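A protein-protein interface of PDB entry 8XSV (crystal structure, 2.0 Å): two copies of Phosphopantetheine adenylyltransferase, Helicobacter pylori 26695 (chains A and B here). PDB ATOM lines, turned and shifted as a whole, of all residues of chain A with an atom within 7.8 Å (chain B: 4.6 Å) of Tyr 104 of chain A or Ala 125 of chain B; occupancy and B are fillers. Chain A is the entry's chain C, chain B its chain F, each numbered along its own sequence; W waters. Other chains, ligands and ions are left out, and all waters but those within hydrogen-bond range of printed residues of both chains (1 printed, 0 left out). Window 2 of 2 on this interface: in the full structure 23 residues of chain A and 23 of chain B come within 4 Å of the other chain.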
ATOM      1  N   GLU A  97      22.100 -21.096 -13.181  1.00  0.00           N
ATOM      2  CA  GLU A  97      21.881 -22.105 -12.182  1.00  0.00           C
ATOM      3  C   GLU A  97      22.998 -23.177 -12.310  1.00  0.00           C
ATOM      4  O   GLU A  97      23.461 -23.673 -11.300  1.00  0.00           O
ATOM      5  CB  GLU A  97      20.457 -22.700 -12.315  1.00  0.00           C
ATOM      6  CG  GLU A  97      19.381 -21.666 -12.113  1.00  0.00           C
ATOM      7  CD  GLU A  97      18.980 -20.933 -13.437  1.00  0.00           C
ATOM      8  OE1 GLU A  97      17.987 -20.155 -13.389  1.00  0.00           O
ATOM      9  OE2 GLU A  97      19.611 -21.120 -14.553  1.00  0.00           O
ATOM     10  N   TYR A  98      23.404 -23.487 -13.540  1.00  0.00           N
ATOM     11  CA  TYR A  98      24.520 -24.355 -13.727  1.00  0.00           C
ATOM     12  C   TYR A  98      25.870 -23.797 -13.201  1.00  0.00           C
ATOM     13  O   TYR A  98      26.653 -24.565 -12.625  1.00  0.00           O
ATOM     14  CB  TYR A  98      24.558 -24.985 -15.153  1.00  0.00           C
ATOM     15  CG  TYR A  98      25.912 -25.205 -15.747  1.00  0.00           C
ATOM     16  CD1 TYR A  98      26.606 -24.133 -16.297  1.00  0.00           C
ATOM     17  CD2 TYR A  98      26.518 -26.502 -15.803  1.00  0.00           C
ATOM     18  CE1 TYR A  98      27.861 -24.298 -16.860  1.00  0.00           C
ATOM     19  CE2 TYR A  98      27.781 -26.676 -16.351  1.00  0.00           C
ATOM     20  CZ  TYR A  98      28.438 -25.562 -16.894  1.00  0.00           C
ATOM     21  OH  TYR A  98      29.698 -25.610 -17.507  1.00  0.00           O
ATOM     22  N   GLU A  99      26.113 -22.490 -13.364  1.00  0.00           N
ATOM     23  CA  GLU A  99      27.250 -21.821 -12.721  1.00  0.00           C
ATOM     24  C   GLU A  99      27.208 -22.015 -11.221  1.00  0.00           C
ATOM     25  O   GLU A  99      28.261 -22.406 -10.657  1.00  0.00           O
ATOM     26  CB  GLU A  99      27.308 -20.296 -12.996  1.00  0.00           C
ATOM     27  CG  GLU A  99      27.512 -20.062 -14.500  1.00  0.00           C
ATOM     28  CD  GLU A  99      28.937 -20.403 -14.916  1.00  0.00           C
ATOM     29  OE1 GLU A  99      29.902 -20.521 -14.084  1.00  0.00           O
ATOM     30  OE2 GLU A  99      29.144 -20.628 -16.109  1.00  0.00           O
ATOM     31  N   LEU A 100      26.053 -21.756 -10.571  1.00  0.00           N
ATOM     32  CA  LEU A 100      25.981 -21.958  -9.111  1.00  0.00           C
ATOM     33  C   LEU A 100      26.261 -23.470  -8.806  1.00  0.00           C
ATOM     34  O   LEU A 100      26.948 -23.800  -7.834  1.00  0.00           O
ATOM     35  CB  LEU A 100      24.607 -21.647  -8.561  1.00  0.00           C
ATOM     36  CG  LEU A 100      24.099 -20.150  -8.677  1.00  0.00           C
ATOM     37  CD1 LEU A 100      22.742 -20.008  -8.026  1.00  0.00           C
ATOM     38  CD2 LEU A 100      25.131 -19.221  -7.937  1.00  0.00           C
ATOM     39  N   GLN A 101      25.648 -24.368  -9.565  1.00  0.00           N
ATOM     40  CA  GLN A 101      25.845 -25.775  -9.282  1.00  0.00           C
ATOM     41  C   GLN A 101      27.353 -26.193  -9.352  1.00  0.00           C
ATOM     42  O   GLN A 101      27.854 -26.897  -8.510  1.00  0.00           O
ATOM     43  CB  GLN A 101      24.937 -26.548 -10.228  1.00  0.00           C
ATOM     44  CG  GLN A 101      25.258 -27.986 -10.257  1.00  0.00           C
ATOM     45  CD  GLN A 101      24.482 -28.792 -11.337  1.00  0.00           C
ATOM     46  OE1 GLN A 101      23.533 -29.523 -11.019  1.00  0.00           O
ATOM     47  NE2 GLN A 101      24.901 -28.675 -12.575  1.00  0.00           N
ATOM     48  N   MET A 102      28.042 -25.759 -10.402  1.00  0.00           N
ATOM     49  CA  MET A 102      29.425 -26.069 -10.606  1.00  0.00           C
ATOM     50  C   MET A 102      30.277 -25.410  -9.474  1.00  0.00           C
ATOM     51  O   MET A 102      31.225 -26.042  -8.972  1.00  0.00           O
ATOM     52  CB  MET A 102      29.821 -25.553 -11.959  1.00  0.00           C
ATOM     53  CG  MET A 102      31.184 -25.954 -12.409  1.00  0.00           C
ATOM     54  SD  MET A 102      31.368 -25.999 -14.225  1.00  0.00           S
ATOM     55  CE  MET A 102      31.081 -24.268 -14.646  1.00  0.00           C
ATOM     56  N   GLY A 103      29.972 -24.173  -9.105  1.00  0.00           N
ATOM     57  CA  GLY A 103      30.684 -23.467  -7.923  1.00  0.00           C
ATOM     58  C   GLY A 103      30.588 -24.303  -6.627  1.00  0.00           C
ATOM     59  O   GLY A 103      31.617 -24.563  -5.861  1.00  0.00           O
ATOM     60  N   TYR A 104      29.373 -24.772  -6.347  1.00  0.00           N
ATOM     61  CA  TYR A 104      29.227 -25.662  -5.118  1.00  0.00           C
ATOM     62  C   TYR A 104      29.896 -26.959  -5.342  1.00  0.00           C
ATOM     63  O   TYR A 104      30.389 -27.535  -4.416  1.00  0.00           O
ATOM     64  CB  TYR A 104      27.712 -25.866  -4.800  1.00  0.00           C
ATOM     65  CG  TYR A 104      27.095 -24.591  -4.313  1.00  0.00           C
ATOM     66  CD1 TYR A 104      27.741 -23.833  -3.301  1.00  0.00           C
ATOM     67  CD2 TYR A 104      25.927 -24.063  -4.907  1.00  0.00           C
ATOM     68  CE1 TYR A 104      27.240 -22.635  -2.855  1.00  0.00           C
ATOM     69  CE2 TYR A 104      25.395 -22.837  -4.493  1.00  0.00           C
ATOM     70  CZ  TYR A 104      26.017 -22.143  -3.417  1.00  0.00           C
ATOM     71  OH  TYR A 104      25.526 -20.903  -2.992  1.00  0.00           O
ATOM     72  N   ALA A 105      29.830 -27.502  -6.575  1.00  0.00           N
ATOM     73  CA  ALA A 105      30.510 -28.804  -6.728  1.00  0.00           C
ATOM     74  C   ALA A 105      32.014 -28.667  -6.565  1.00  0.00           C
ATOM     75  O   ALA A 105      32.637 -29.518  -5.908  1.00  0.00           O
ATOM     76  CB  ALA A 105      30.193 -29.408  -8.061  1.00  0.00           C
ATOM     77  N   ASN A 106      32.620 -27.657  -7.205  1.00  0.00           N
ATOM     78  CA  ASN A 106      34.042 -27.402  -6.992  1.00  0.00           C
ATOM     79  C   ASN A 106      34.393 -27.147  -5.502  1.00  0.00           C
ATOM     80  O   ASN A 106      35.479 -27.548  -5.008  1.00  0.00           O
ATOM     81  CB  ASN A 106      34.515 -26.194  -7.822  1.00  0.00           C
ATOM     82  CG  ASN A 106      34.616 -26.519  -9.298  1.00  0.00           C
ATOM     83  OD1 ASN A 106      34.272 -25.656 -10.210  1.00  0.00           O
ATOM     84  ND2 ASN A 106      34.979 -27.687  -9.577  1.00  0.00           N
ATOM     85  N   LYS A 107      33.537 -26.410  -4.798  1.00  0.00           N
ATOM     86  CA  LYS A 107      33.811 -26.285  -3.371  1.00  0.00           C
ATOM     87  C   LYS A 107      33.698 -27.594  -2.548  1.00  0.00           C
ATOM     88  O   LYS A 107      34.375 -27.753  -1.541  1.00  0.00           O
ATOM     89  CB  LYS A 107      32.982 -25.217  -2.764  1.00  0.00           C
ATOM     90  CG  LYS A 107      33.448 -25.125  -1.344  1.00  0.00           C
ATOM     91  CD  LYS A 107      32.787 -24.079  -0.583  1.00  0.00           C
ATOM     92  CE  LYS A 107      33.720 -22.863  -0.755  1.00  0.00           C
ATOM     93  NZ  LYS A 107      32.940 -21.765  -0.103  1.00  0.00           N
ATOM     94  N   SER A 108      32.830 -28.527  -2.982  1.00  0.00           N
ATOM     95  CA  SER A 108      32.678 -29.796  -2.311  1.00  0.00           C
ATOM     96  C   SER A 108      33.879 -30.740  -2.591  1.00  0.00           C
ATOM     97  O   SER A 108      34.239 -31.542  -1.706  1.00  0.00           O
ATOM     98  CB  SER A 108      31.367 -30.418  -2.790  1.00  0.00           C
ATOM     99  OG  SER A 108      31.605 -31.005  -4.084  1.00  0.00           O
ATOM    100  N   LEU A 109      34.513 -30.572  -3.768  1.00  0.00           N
ATOM    101  CA  LEU A 109      35.793 -31.160  -4.096  1.00  0.00           C
ATOM    102  C   LEU A 109      37.040 -30.494  -3.464  1.00  0.00           C
ATOM    103  O   LEU A 109      38.095 -31.108  -3.401  1.00  0.00           O
ATOM    104  CB  LEU A 109      35.988 -31.137  -5.613  1.00  0.00           C
ATOM    105  CG  LEU A 109      34.845 -31.938  -6.322  1.00  0.00           C
ATOM    106  CD1 LEU A 109      34.919 -31.650  -7.829  1.00  0.00           C
ATOM    107  CD2 LEU A 109      35.022 -33.444  -6.061  1.00  0.00           C
ATOM    108  N   ASN A 110      36.924 -29.265  -2.993  1.00  0.00           N
ATOM    109  CA  ASN A 110      38.092 -28.572  -2.425  1.00  0.00           C
ATOM    110  C   ASN A 110      37.546 -27.451  -1.531  1.00  0.00           C
ATOM    111  O   ASN A 110      37.097 -26.405  -2.046  1.00  0.00           O
ATOM    112  CB  ASN A 110      38.954 -28.007  -3.579  1.00  0.00           C
ATOM    113  CG  ASN A 110      40.136 -27.189  -3.073  1.00  0.00           C
ATOM    114  OD1 ASN A 110      40.236 -26.921  -1.893  1.00  0.00           O
ATOM    115  ND2 ASN A 110      41.055 -26.826  -3.968  1.00  0.00           N
ATOM    116  N   HIS A 111      37.599 -27.649  -0.196  1.00  0.00           N
ATOM    117  CA  HIS A 111      36.848 -26.864   0.707  1.00  0.00           C
ATOM    118  C   HIS A 111      37.328 -25.481   0.794  1.00  0.00           C
ATOM    119  O   HIS A 111      36.658 -24.720   1.402  1.00  0.00           O
ATOM    120  CB  HIS A 111      36.808 -27.513   2.087  1.00  0.00           C
ATOM    121  CG  HIS A 111      36.034 -28.829   2.076  1.00  0.00           C
ATOM    122  ND1 HIS A 111      36.280 -29.836   2.968  1.00  0.00           N
ATOM    123  CD2 HIS A 111      35.047 -29.319   1.179  1.00  0.00           C
ATOM    124  CE1 HIS A 111      35.492 -30.915   2.665  1.00  0.00           C
ATOM    125  NE2 HIS A 111      34.732 -30.600   1.576  1.00  0.00           N
ATOM    126  N   LEU A 113      37.935 -23.671  -1.951  1.00  0.00           N
ATOM    127  CA  LEU A 113      37.904 -23.060  -3.256  1.00  0.00           C
ATOM    128  C   LEU A 113      36.602 -22.295  -3.558  1.00  0.00           C
ATOM    129  O   LEU A 113      35.509 -22.893  -3.682  1.00  0.00           O
ATOM    130  CB  LEU A 113      38.115 -24.124  -4.297  1.00  0.00           C
ATOM    131  CG  LEU A 113      38.319 -23.750  -5.771  1.00  0.00           C
ATOM    132  CD1 LEU A 113      39.500 -22.802  -5.988  1.00  0.00           C
ATOM    133  CD2 LEU A 113      38.546 -25.020  -6.558  1.00  0.00           C
ATOM    134  N   GLU A 114      36.738 -20.999  -3.703  1.00  0.00           N
ATOM    135  CA  GLU A 114      35.615 -20.096  -3.951  1.00  0.00           C
ATOM    136  C   GLU A 114      35.451 -19.918  -5.421  1.00  0.00           C
ATOM    137  O   GLU A 114      36.405 -20.202  -6.240  1.00  0.00           O
ATOM    138  CB  GLU A 114      35.959 -18.738  -3.391  1.00  0.00           C
ATOM    139  CG  GLU A 114      36.299 -18.739  -1.882  1.00  0.00           C
ATOM    140  CD  GLU A 114      35.222 -19.517  -1.039  1.00  0.00           C
ATOM    141  OE1 GLU A 114      33.995 -19.493  -1.277  1.00  0.00           O
ATOM    142  OE2 GLU A 114      35.608 -20.040  -0.027  1.00  0.00           O
ATOM    143  N   THR A 115      34.249 -19.454  -5.810  1.00  0.00           N
ATOM    144  CA  THR A 115      34.064 -19.021  -7.266  1.00  0.00           C
ATOM    145  C   THR A 115      33.622 -17.597  -7.265  1.00  0.00           C
ATOM    146  O   THR A 115      32.730 -17.218  -6.532  1.00  0.00           O
ATOM    147  CB  THR A 115      33.063 -19.924  -8.049  1.00  0.00           C
ATOM    148  OG1 THR A 115      33.511 -21.296  -8.039  1.00  0.00           O
ATOM    149  CG2 THR A 115      32.889 -19.473  -9.479  1.00  0.00           C
ATOM    150  N   TYR A 117      32.615 -14.170  -9.885  1.00  0.00           N
ATOM    151  CA  TYR A 117      32.187 -13.933 -11.274  1.00  0.00           C
ATOM    152  C   TYR A 117      32.382 -12.506 -11.677  1.00  0.00           C
ATOM    153  O   TYR A 117      32.022 -11.636 -10.860  1.00  0.00           O
ATOM    154  CB  TYR A 117      30.613 -14.227 -11.390  1.00  0.00           C
ATOM    155  CG  TYR A 117      30.271 -15.691 -11.008  1.00  0.00           C
ATOM    156  CD1 TYR A 117      30.223 -16.670 -11.967  1.00  0.00           C
ATOM    157  CD2 TYR A 117      29.940 -16.017  -9.702  1.00  0.00           C
ATOM    158  CE1 TYR A 117      29.929 -17.986 -11.658  1.00  0.00           C
ATOM    159  CE2 TYR A 117      29.601 -17.279  -9.363  1.00  0.00           C
ATOM    160  CZ  TYR A 117      29.590 -18.273 -10.362  1.00  0.00           C
ATOM    161  OH  TYR A 117      29.247 -19.563 -10.011  1.00  0.00           O
ATOM    162  N   ARG B  91      22.304 -15.736  -5.832  1.00  0.00           N
ATOM    163  CA  ARG B  91      21.613 -16.869  -5.201  1.00  0.00           C
ATOM    164  C   ARG B  91      20.604 -17.468  -6.162  1.00  0.00           C
ATOM    165  O   ARG B  91      20.520 -17.052  -7.383  1.00  0.00           O
ATOM    166  CB  ARG B  91      20.912 -16.425  -3.903  1.00  0.00           C
ATOM    167  CG  ARG B  91      20.565 -14.926  -3.833  1.00  0.00           C
ATOM    168  CD  ARG B  91      19.274 -14.638  -4.539  1.00  0.00           C
ATOM    169  NE  ARG B  91      18.813 -13.229  -4.336  1.00  0.00           N
ATOM    170  CZ  ARG B  91      17.984 -12.838  -3.374  1.00  0.00           C
ATOM    171  NH1 ARG B  91      17.553 -11.570  -3.283  1.00  0.00           N
ATOM    172  NH2 ARG B  91      17.586 -13.724  -2.499  1.00  0.00           N
ATOM    173  N   VAL B  92      19.827 -18.411  -5.626  1.00  0.00           N
ATOM    174  CA  VAL B  92      18.981 -19.280  -6.512  1.00  0.00           C
ATOM    175  C   VAL B  92      17.901 -18.399  -7.120  1.00  0.00           C
ATOM    176  O   VAL B  92      17.530 -18.566  -8.296  1.00  0.00           O
ATOM    177  CB  VAL B  92      18.327 -20.471  -5.714  1.00  0.00           C
ATOM    178  CG1 VAL B  92      17.201 -21.185  -6.557  1.00  0.00           C
ATOM    179  CG2 VAL B  92      19.374 -21.538  -5.427  1.00  0.00           C
ATOM    180  N   MET B 119      29.009 -16.039  -4.208  1.00  0.00           N
ATOM    181  CA  MET B 119      27.949 -16.947  -3.876  1.00  0.00           C
ATOM    182  C   MET B 119      27.995 -17.150  -2.337  1.00  0.00           C
ATOM    183  O   MET B 119      29.034 -17.259  -1.772  1.00  0.00           O
ATOM    184  CB  MET B 119      28.051 -18.360  -4.510  1.00  0.00           C
ATOM    185  CG  MET B 119      28.497 -18.341  -5.999  1.00  0.00           C
ATOM    186  SD  MET B 119      29.212 -19.913  -6.458  1.00  0.00           S
ATOM    187  CE  MET B 119      28.224 -21.074  -5.584  1.00  0.00           C
ATOM    188  N   PRO B 120      26.809 -17.322  -1.740  1.00  0.00           N
ATOM    189  CA  PRO B 120      26.691 -17.663  -0.318  1.00  0.00           C
ATOM    190  C   PRO B 120      26.952 -19.136  -0.136  1.00  0.00           C
ATOM    191  O   PRO B 120      27.139 -19.881  -1.077  1.00  0.00           O
ATOM    192  CB  PRO B 120      25.185 -17.299  -0.053  1.00  0.00           C
ATOM    193  CG  PRO B 120      24.480 -17.722  -1.360  1.00  0.00           C
ATOM    194  CD  PRO B 120      25.498 -17.390  -2.452  1.00  0.00           C
ATOM    195  N   THR B 121      26.996 -19.588   1.110  1.00  0.00           N
ATOM    196  CA  THR B 121      27.064 -21.025   1.377  1.00  0.00           C
ATOM    197  C   THR B 121      25.809 -21.652   0.709  1.00  0.00           C
ATOM    198  O   THR B 121      24.726 -21.010   0.582  1.00  0.00           O
ATOM    199  CB  THR B 121      27.068 -21.412   2.891  1.00  0.00           C
ATOM    200  OG1 THR B 121      25.865 -20.955   3.501  1.00  0.00           O
ATOM    201  CG2 THR B 121      28.277 -20.803   3.680  1.00  0.00           C
ATOM    202  N   LEU B 122      25.939 -22.899   0.341  1.00  0.00           N
ATOM    203  CA  LEU B 122      24.820 -23.559  -0.365  1.00  0.00           C
ATOM    204  C   LEU B 122      23.553 -23.544   0.522  1.00  0.00           C
ATOM    205  O   LEU B 122      22.403 -23.333   0.013  1.00  0.00           O
ATOM    206  CB  LEU B 122      25.286 -25.017  -0.587  1.00  0.00           C
ATOM    207  CG  LEU B 122      24.336 -25.820  -1.421  1.00  0.00           C
ATOM    208  CD1 LEU B 122      25.033 -27.057  -1.958  1.00  0.00           C
ATOM    209  CD2 LEU B 122      23.173 -26.363  -0.546  1.00  0.00           C
ATOM    210  N   GLN B 123      23.745 -23.774   1.831  1.00  0.00           N
ATOM    211  CA  GLN B 123      22.577 -23.786   2.764  1.00  0.00           C
ATOM    212  C   GLN B 123      21.837 -22.461   2.764  1.00  0.00           C
ATOM    213  O   GLN B 123      20.636 -22.473   2.994  1.00  0.00           O
ATOM    214  CB  GLN B 123      22.963 -24.179   4.229  1.00  0.00           C
ATOM    215  CG  GLN B 123      23.078 -25.736   4.447  1.00  0.00           C
ATOM    216  CD  GLN B 123      21.703 -26.501   4.519  1.00  0.00           C
ATOM    217  OE1 GLN B 123      21.579 -27.637   4.022  1.00  0.00           O
ATOM    218  NE2 GLN B 123      20.701 -25.870   5.091  1.00  0.00           N
ATOM    219  N   ASN B 124      22.517 -21.322   2.547  1.00  0.00           N
ATOM    220  CA  ASN B 124      21.823 -20.033   2.587  1.00  0.00           C
ATOM    221  C   ASN B 124      21.442 -19.514   1.197  1.00  0.00           C
ATOM    222  O   ASN B 124      20.964 -18.406   1.072  1.00  0.00           O
ATOM    223  CB  ASN B 124      22.652 -19.008   3.349  1.00  0.00           C
ATOM    224  CG  ASN B 124      22.846 -19.382   4.812  1.00  0.00           C
ATOM    225  OD1 ASN B 124      23.876 -18.983   5.440  1.00  0.00           O
ATOM    226  ND2 ASN B 124      22.005 -20.238   5.324  1.00  0.00           N
ATOM    227  N   ALA B 125      21.633 -20.335   0.175  1.00  0.00           N
ATOM    228  CA  ALA B 125      21.415 -19.906  -1.199  1.00  0.00           C
ATOM    229  C   ALA B 125      19.891 -19.745  -1.567  1.00  0.00           C
ATOM    230  O   ALA B 125      19.617 -19.069  -2.502  1.00  0.00           O
ATOM    231  CB  ALA B 125      22.087 -20.863  -2.124  1.00  0.00           C
ATOM    232  N   PHE B 126      18.982 -20.246  -0.716  1.00  0.00           N
ATOM    233  CA  PHE B 126      17.553 -20.036  -0.870  1.00  0.00           C
ATOM    234  C   PHE B 126      16.953 -19.003   0.074  1.00  0.00           C
ATOM    235  O   PHE B 126      15.743 -18.868   0.106  1.00  0.00           O
ATOM    236  CB  PHE B 126      16.761 -21.356  -0.631  1.00  0.00           C
ATOM    237  CG  PHE B 126      17.019 -22.390  -1.696  1.00  0.00           C
ATOM    238  CD1 PHE B 126      17.949 -23.342  -1.501  1.00  0.00           C
ATOM    239  CD2 PHE B 126      16.415 -22.266  -2.954  1.00  0.00           C
ATOM    240  CE1 PHE B 126      18.189 -24.308  -2.507  1.00  0.00           C
ATOM    241  CE2 PHE B 126      16.601 -23.228  -3.935  1.00  0.00           C
ATOM    242  CZ  PHE B 126      17.536 -24.215  -3.695  1.00  0.00           C
ATOM    243  N   ILE B 127      17.766 -18.326   0.875  1.00  0.00           N
ATOM    244  CA  ILE B 127      17.290 -17.328   1.836  1.00  0.00           C
ATOM    245  C   ILE B 127      17.019 -16.012   1.113  1.00  0.00           C
ATOM    246  O   ILE B 127      17.886 -15.450   0.470  1.00  0.00           O
ATOM    247  CB  ILE B 127      18.363 -17.103   2.965  1.00  0.00           C
ATOM    248  CG1 ILE B 127      18.489 -18.326   3.908  1.00  0.00           C
ATOM    249  CG2 ILE B 127      17.913 -15.950   3.865  1.00  0.00           C
ATOM    250  CD1 ILE B 127      19.182 -18.023   5.230  1.00  0.00           C
HETATM  251  O   HOH W   1      31.816 -16.760  -3.938  1.00  0.00           O
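OH of Tyr 104 of chain A sits at hydrogen-bond distance from O of Pro 120 of chain B, 2.7 Å away.
OH of Tyr 117 of chain A lies within hydrogen-bond range of SD of Met 119 of chain B (3.6 Å).
The side-chain hydroxyl of Tyr 117 of chain A lies within hydrogen-bond range of the backbone carbonyl oxygen of Glu 99 of chain A (3.1 Å).
The guanidinium group (NH2) of Arg 91 of chain B sits at hydrogen-bond distance from the backbone carbonyl oxygen (O) of Ile 127 of chain B, at 3.4 Å.
The side-chain amide oxygen (OD1) of Asn 124 of chain B lies within hydrogen-bond range of the side-chain hydroxyl (OG1) of Thr 121 of chain B.
N of Val 92 of chain B is in hydrogen-bond range of O of Ala 125 of chain B (3.2 Å).
Leu 100 of chain A touches Arg 91 of chain B.
Met 119 of chain B touches Leu 100 of chain A (CE to O, 3.8 Å).
Tyr 104 of chain A touches Met 119 of chain B.
Tyr 104 of chain A touches Thr 121 of chain B.
Leu 122 of chain B touches Tyr 104 of chain A (N to CE1, 3.5 Å).
CB of Ala 125 of chain B touches OH of Tyr 104 of chain A, at 3.5 Å.
Tyr 104 of chain A touches just these residues of chain B: Met 119 (3.3 Å), Pro 120 (2.7 Å), Thr 121 (3.7 Å), Leu 122 (3.5 Å) and Ala 125 (3.5 Å).
Printed residues of chain A within 4 Å of Pro 120 of chain B: Tyr 104 (2.7 Å).
Printed residues of chain A within 4 Å of Thr 121 of chain B: Tyr 104 (3.7 Å).
Of the printed residues of chain A, Leu 122 of chain B touches Tyr 104 (3.5 Å).
Ala 125 of chain B touches just one residue of chain A: Tyr 104.
The nearest residue of chain A that does not touch Ala 125 of chain B is Leu 100 of chain A (6.0 Å).
Hydrophobic or aromatic side chains of chain A that line the printed part of chain B: Leu 100, Tyr 104 and Tyr 117.
Printed residues of chain B that touch a printed residue of chain A: Arg 91, Met 119, Pro 120, Thr 121, Leu 122 and Ala 125.
Hydrophobic or aromatic side chains of chain B within 4 Å of the printed part of chain A: Met 119, Pro 120, Leu 122 and Ala 125.
No position is printed for both chains.
Of the 8 pairs that touch across the chains among the printed residues, none has its exchanged pair printed and touching as well.
Water W1 bridges the backbone carbonyl oxygen (O) of Thr 115 of chain A (2.8 Å) and the backbone NH (N) of Met 119 of chain B (2.9 Å).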
